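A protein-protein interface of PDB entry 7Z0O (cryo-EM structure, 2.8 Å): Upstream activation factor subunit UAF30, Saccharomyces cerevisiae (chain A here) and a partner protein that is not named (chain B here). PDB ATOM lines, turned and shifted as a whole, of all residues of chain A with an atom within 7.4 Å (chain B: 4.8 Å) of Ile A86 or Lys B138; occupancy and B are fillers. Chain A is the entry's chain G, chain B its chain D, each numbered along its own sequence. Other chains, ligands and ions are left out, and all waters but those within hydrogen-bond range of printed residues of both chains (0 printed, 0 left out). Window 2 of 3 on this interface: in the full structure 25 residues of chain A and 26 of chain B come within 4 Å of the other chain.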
ATOM      1  N   GLU A  81       0.935  -1.669  14.389  1.00  0.00           N
ATOM      2  CA  GLU A  81       1.499  -2.029  15.684  1.00  0.00           C
ATOM      3  C   GLU A  81       3.021  -2.066  15.615  1.00  0.00           C
ATOM      4  O   GLU A  81       3.699  -1.577  16.526  1.00  0.00           O
ATOM      5  CB  GLU A  81       0.874  -3.361  16.141  1.00  0.00           C
ATOM      6  CG  GLU A  81       1.177  -3.949  17.552  1.00  0.00           C
ATOM      7  CD  GLU A  81       2.634  -4.226  17.915  1.00  0.00           C
ATOM      8  OE1 GLU A  81       3.521  -4.221  17.045  1.00  0.00           O
ATOM      9  OE2 GLU A  81       2.892  -4.452  19.116  1.00  0.00           O
ATOM     10  N   LEU A  82       3.575  -2.622  14.535  1.00  0.00           N
ATOM     11  CA  LEU A  82       5.026  -2.720  14.413  1.00  0.00           C
ATOM     12  C   LEU A  82       5.683  -1.350  14.315  1.00  0.00           C
ATOM     13  O   LEU A  82       6.830  -1.186  14.744  1.00  0.00           O
ATOM     14  CB  LEU A  82       5.398  -3.569  13.198  1.00  0.00           C
ATOM     15  CG  LEU A  82       5.298  -5.085  13.375  1.00  0.00           C
ATOM     16  CD1 LEU A  82       5.927  -5.803  12.197  1.00  0.00           C
ATOM     17  CD2 LEU A  82       5.956  -5.510  14.673  1.00  0.00           C
ATOM     18  N   THR A  83       4.987  -0.364  13.751  1.00  0.00           N
ATOM     19  CA  THR A  83       5.555   0.977  13.663  1.00  0.00           C
ATOM     20  C   THR A  83       5.665   1.622  15.039  1.00  0.00           C
ATOM     21  O   THR A  83       6.565   2.435  15.279  1.00  0.00           O
ATOM     22  CB  THR A  83       4.713   1.847  12.733  1.00  0.00           C
ATOM     23  OG1 THR A  83       3.331   1.736  13.093  1.00  0.00           O
ATOM     24  CG2 THR A  83       4.893   1.408  11.288  1.00  0.00           C
ATOM     25  N   LYS A  84       4.757   1.278  15.953  1.00  0.00           N
ATOM     26  CA  LYS A  84       4.796   1.843  17.297  1.00  0.00           C
ATOM     27  C   LYS A  84       6.039   1.430  18.073  1.00  0.00           C
ATOM     28  O   LYS A  84       6.607   2.263  18.786  1.00  0.00           O
ATOM     29  CB  LYS A  84       3.539   1.449  18.076  1.00  0.00           C
ATOM     30  CG  LYS A  84       2.227   1.900  17.442  1.00  0.00           C
ATOM     31  CD  LYS A  84       2.373   3.247  16.741  1.00  0.00           C
ATOM     32  CE  LYS A  84       1.355   3.411  15.624  1.00  0.00           C
ATOM     33  NZ  LYS A  84       0.033   3.872  16.134  1.00  0.00           N
ATOM     34  N   GLU A  85       6.477   0.173  17.956  1.00  0.00           N
ATOM     35  CA  GLU A  85       7.684  -0.245  18.662  1.00  0.00           C
ATOM     36  C   GLU A  85       8.918   0.467  18.123  1.00  0.00           C
ATOM     37  O   GLU A  85       9.951   0.534  18.801  1.00  0.00           O
ATOM     38  CB  GLU A  85       7.861  -1.761  18.577  1.00  0.00           C
ATOM     39  CG  GLU A  85       6.578  -2.564  18.669  1.00  0.00           C
ATOM     40  CD  GLU A  85       6.806  -4.038  18.401  1.00  0.00           C
ATOM     41  OE1 GLU A  85       7.978  -4.436  18.233  1.00  0.00           O
ATOM     42  OE2 GLU A  85       5.822  -4.805  18.373  1.00  0.00           O
ATOM     43  N   ILE A  86       8.838   0.998  16.909  1.00  0.00           N
ATOM     44  CA  ILE A  86       9.936   1.768  16.343  1.00  0.00           C
ATOM     45  C   ILE A  86       9.716   3.253  16.602  1.00  0.00           C
ATOM     46  O   ILE A  86       9.954   3.743  17.706  1.00  0.00           O
ATOM     47  CB  ILE A  86      10.093   1.495  14.843  1.00  0.00           C
ATOM     48  CG1 ILE A  86      10.579   0.067  14.610  1.00  0.00           C
ATOM     49  CG2 ILE A  86      11.061   2.485  14.224  1.00  0.00           C
ATOM     50  CD1 ILE A  86      10.691  -0.297  13.152  1.00  0.00           C
ATOM     51  N   GLN B   6      12.834  -6.317  15.453  1.00  0.00           N
ATOM     52  CA  GLN B   6      12.541  -6.240  14.025  1.00  0.00           C
ATOM     53  C   GLN B   6      13.716  -5.683  13.238  1.00  0.00           C
ATOM     54  O   GLN B   6      13.870  -5.993  12.051  1.00  0.00           O
ATOM     55  CB  GLN B   6      11.307  -5.373  13.789  1.00  0.00           C
ATOM     56  CG  GLN B   6      10.342  -5.340  14.952  1.00  0.00           C
ATOM     57  CD  GLN B   6       9.489  -4.091  14.950  1.00  0.00           C
ATOM     58  OE1 GLN B   6       9.418  -3.376  13.951  1.00  0.00           O
ATOM     59  NE2 GLN B   6       8.841  -3.815  16.074  1.00  0.00           N
ATOM     60  N   ALA B 134       5.128   2.007   4.456  1.00  0.00           N
ATOM     61  CA  ALA B 134       5.338   2.959   5.541  1.00  0.00           C
ATOM     62  C   ALA B 134       6.192   2.350   6.644  1.00  0.00           C
ATOM     63  O   ALA B 134       7.074   3.015   7.197  1.00  0.00           O
ATOM     64  CB  ALA B 134       3.995   3.428   6.095  1.00  0.00           C
ATOM     65  N   LEU B 135       5.940   1.083   6.979  1.00  0.00           N
ATOM     66  CA  LEU B 135       6.770   0.400   7.965  1.00  0.00           C
ATOM     67  C   LEU B 135       8.183   0.181   7.441  1.00  0.00           C
ATOM     68  O   LEU B 135       9.161   0.366   8.174  1.00  0.00           O
ATOM     69  CB  LEU B 135       6.131  -0.932   8.354  1.00  0.00           C
ATOM     70  CG  LEU B 135       7.032  -1.918   9.096  1.00  0.00           C
ATOM     71  CD1 LEU B 135       7.381  -1.390  10.474  1.00  0.00           C
ATOM     72  CD2 LEU B 135       6.369  -3.278   9.194  1.00  0.00           C
ATOM     73  N   GLU B 136       8.310  -0.217   6.173  1.00  0.00           N
ATOM     74  CA  GLU B 136       9.628  -0.493   5.613  1.00  0.00           C
ATOM     75  C   GLU B 136      10.472   0.771   5.525  1.00  0.00           C
ATOM     76  O   GLU B 136      11.682   0.736   5.778  1.00  0.00           O
ATOM     77  CB  GLU B 136       9.489  -1.144   4.240  1.00  0.00           C
ATOM     78  CG  GLU B 136      10.784  -1.198   3.459  1.00  0.00           C
ATOM     79  CD  GLU B 136      10.737  -2.205   2.337  1.00  0.00           C
ATOM     80  OE1 GLU B 136       9.832  -3.065   2.353  1.00  0.00           O
ATOM     81  OE2 GLU B 136      11.600  -2.139   1.439  1.00  0.00           O
ATOM     82  N   THR B 137       9.856   1.898   5.160  1.00  0.00           N
ATOM     83  CA  THR B 137      10.596   3.155   5.121  1.00  0.00           C
ATOM     84  C   THR B 137      11.123   3.521   6.501  1.00  0.00           C
ATOM     85  O   THR B 137      12.252   4.008   6.633  1.00  0.00           O
ATOM     86  CB  THR B 137       9.715   4.276   4.573  1.00  0.00           C
ATOM     87  OG1 THR B 137       8.416   4.202   5.171  1.00  0.00           O
ATOM     88  CG2 THR B 137       9.583   4.157   3.065  1.00  0.00           C
ATOM     89  N   LYS B 138      10.319   3.299   7.542  1.00  0.00           N
ATOM     90  CA  LYS B 138      10.793   3.529   8.902  1.00  0.00           C
ATOM     91  C   LYS B 138      11.945   2.596   9.248  1.00  0.00           C
ATOM     92  O   LYS B 138      12.927   3.017   9.870  1.00  0.00           O
ATOM     93  CB  LYS B 138       9.645   3.352   9.894  1.00  0.00           C
ATOM     94  CG  LYS B 138       8.707   4.545   9.970  1.00  0.00           C
ATOM     95  CD  LYS B 138       8.173   4.748  11.378  1.00  0.00           C
ATOM     96  CE  LYS B 138       9.281   5.103  12.357  1.00  0.00           C
ATOM     97  NZ  LYS B 138      10.366   5.909  11.730  1.00  0.00           N
ATOM     98  N   LEU B 139      11.839   1.324   8.860  1.00  0.00           N
ATOM     99  CA  LEU B 139      12.917   0.378   9.128  1.00  0.00           C
ATOM    100  C   LEU B 139      14.180   0.744   8.360  1.00  0.00           C
ATOM    101  O   LEU B 139      15.287   0.682   8.907  1.00  0.00           O
ATOM    102  CB  LEU B 139      12.469  -1.040   8.781  1.00  0.00           C
ATOM    103  CG  LEU B 139      11.856  -1.857   9.916  1.00  0.00           C
ATOM    104  CD1 LEU B 139      11.225  -3.126   9.378  1.00  0.00           C
ATOM    105  CD2 LEU B 139      12.908  -2.185  10.956  1.00  0.00           C
ATOM    106  N   SER B 140      14.036   1.118   7.087  1.00  0.00           N
ATOM    107  CA  SER B 140      15.201   1.492   6.292  1.00  0.00           C
ATOM    108  C   SER B 140      15.861   2.753   6.832  1.00  0.00           C
ATOM    109  O   SER B 140      17.091   2.829   6.915  1.00  0.00           O
ATOM    110  CB  SER B 140      14.799   1.689   4.833  1.00  0.00           C
ATOM    111  OG  SER B 140      13.808   2.691   4.712  1.00  0.00           O
ATOM    112  N   GLU B 141      15.059   3.754   7.200  1.00  0.00           N
ATOM    113  CA  GLU B 141      15.617   4.992   7.732  1.00  0.00           C
ATOM    114  C   GLU B 141      16.321   4.752   9.060  1.00  0.00           C
ATOM    115  O   GLU B 141      17.361   5.358   9.338  1.00  0.00           O
ATOM    116  CB  GLU B 141      14.517   6.041   7.888  1.00  0.00           C
ATOM    117  CG  GLU B 141      14.202   6.792   6.610  1.00  0.00           C
ATOM    118  CD  GLU B 141      12.858   7.487   6.661  1.00  0.00           C
ATOM    119  OE1 GLU B 141      12.157   7.351   7.685  1.00  0.00           O
ATOM    120  OE2 GLU B 141      12.505   8.172   5.678  1.00  0.00           O
ATOM    121  N   THR B 142      15.759   3.880   9.899  1.00  0.00           N
ATOM    122  CA  THR B 142      16.416   3.542  11.156  1.00  0.00           C
ATOM    123  C   THR B 142      17.762   2.874  10.909  1.00  0.00           C
ATOM    124  O   THR B 142      18.746   3.174  11.593  1.00  0.00           O
ATOM    125  CB  THR B 142      15.514   2.634  11.990  1.00  0.00           C
ATOM    126  OG1 THR B 142      14.249   3.275  12.194  1.00  0.00           O
ATOM    127  CG2 THR B 142      16.151   2.347  13.337  1.00  0.00           C
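Of chain B, only Gln B6 (3.4 Å), Lys B138 (3.7 Å), Leu B139 (3.6 Å) and Thr B142 (3.9 Å) come within 4 Å of Ile A86. Of chain A, only Ile A86 (3.7 Å) comes within 4 Å of Lys B138. Of the printed residues of chain B, Thr A83 touches Leu B135. Of the printed residues of chain A, Gln B6 touches Leu A82 (3.5 Å), Glu A85 (2.4 Å) and Ile A86 (3.4 Å). Printed residues of chain A within 4 Å of Thr B142: Ile A86 (3.9 Å). Lys A84 touches none of the printed residues of chain B. The nearest residue of chain A that does not touch Lys B138 is Thr A83 (4.7 Å).
OE1 of Glu A81 lies close to OE2 of Glu A85, 2.7 Å away. The side-chain hydroxyl (OG1) of Thr B142 lies within hydrogen-bond range of the backbone carbonyl oxygen (O) of Lys B138 (2.7 Å).
Among the printed residues, merely in contact across the chains: Ile A86 with Gln B6, Ile A86 with Leu B139, Ile A86 with Lys B138, Thr A83 with Leu B135, Ile A86 with Thr B142 and Leu A82 with Leu B135.
OE1 of Gln B6 sits close to O of Leu A82 (3.5 Å). OE1 of Glu A85 is in hydrogen-bond range of NE2 of Gln B6 (2.4 Å).
Hydrophobic or aromatic side chains of chain A within 4 Å of the printed part of chain B: Leu A82 and Ile A86.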
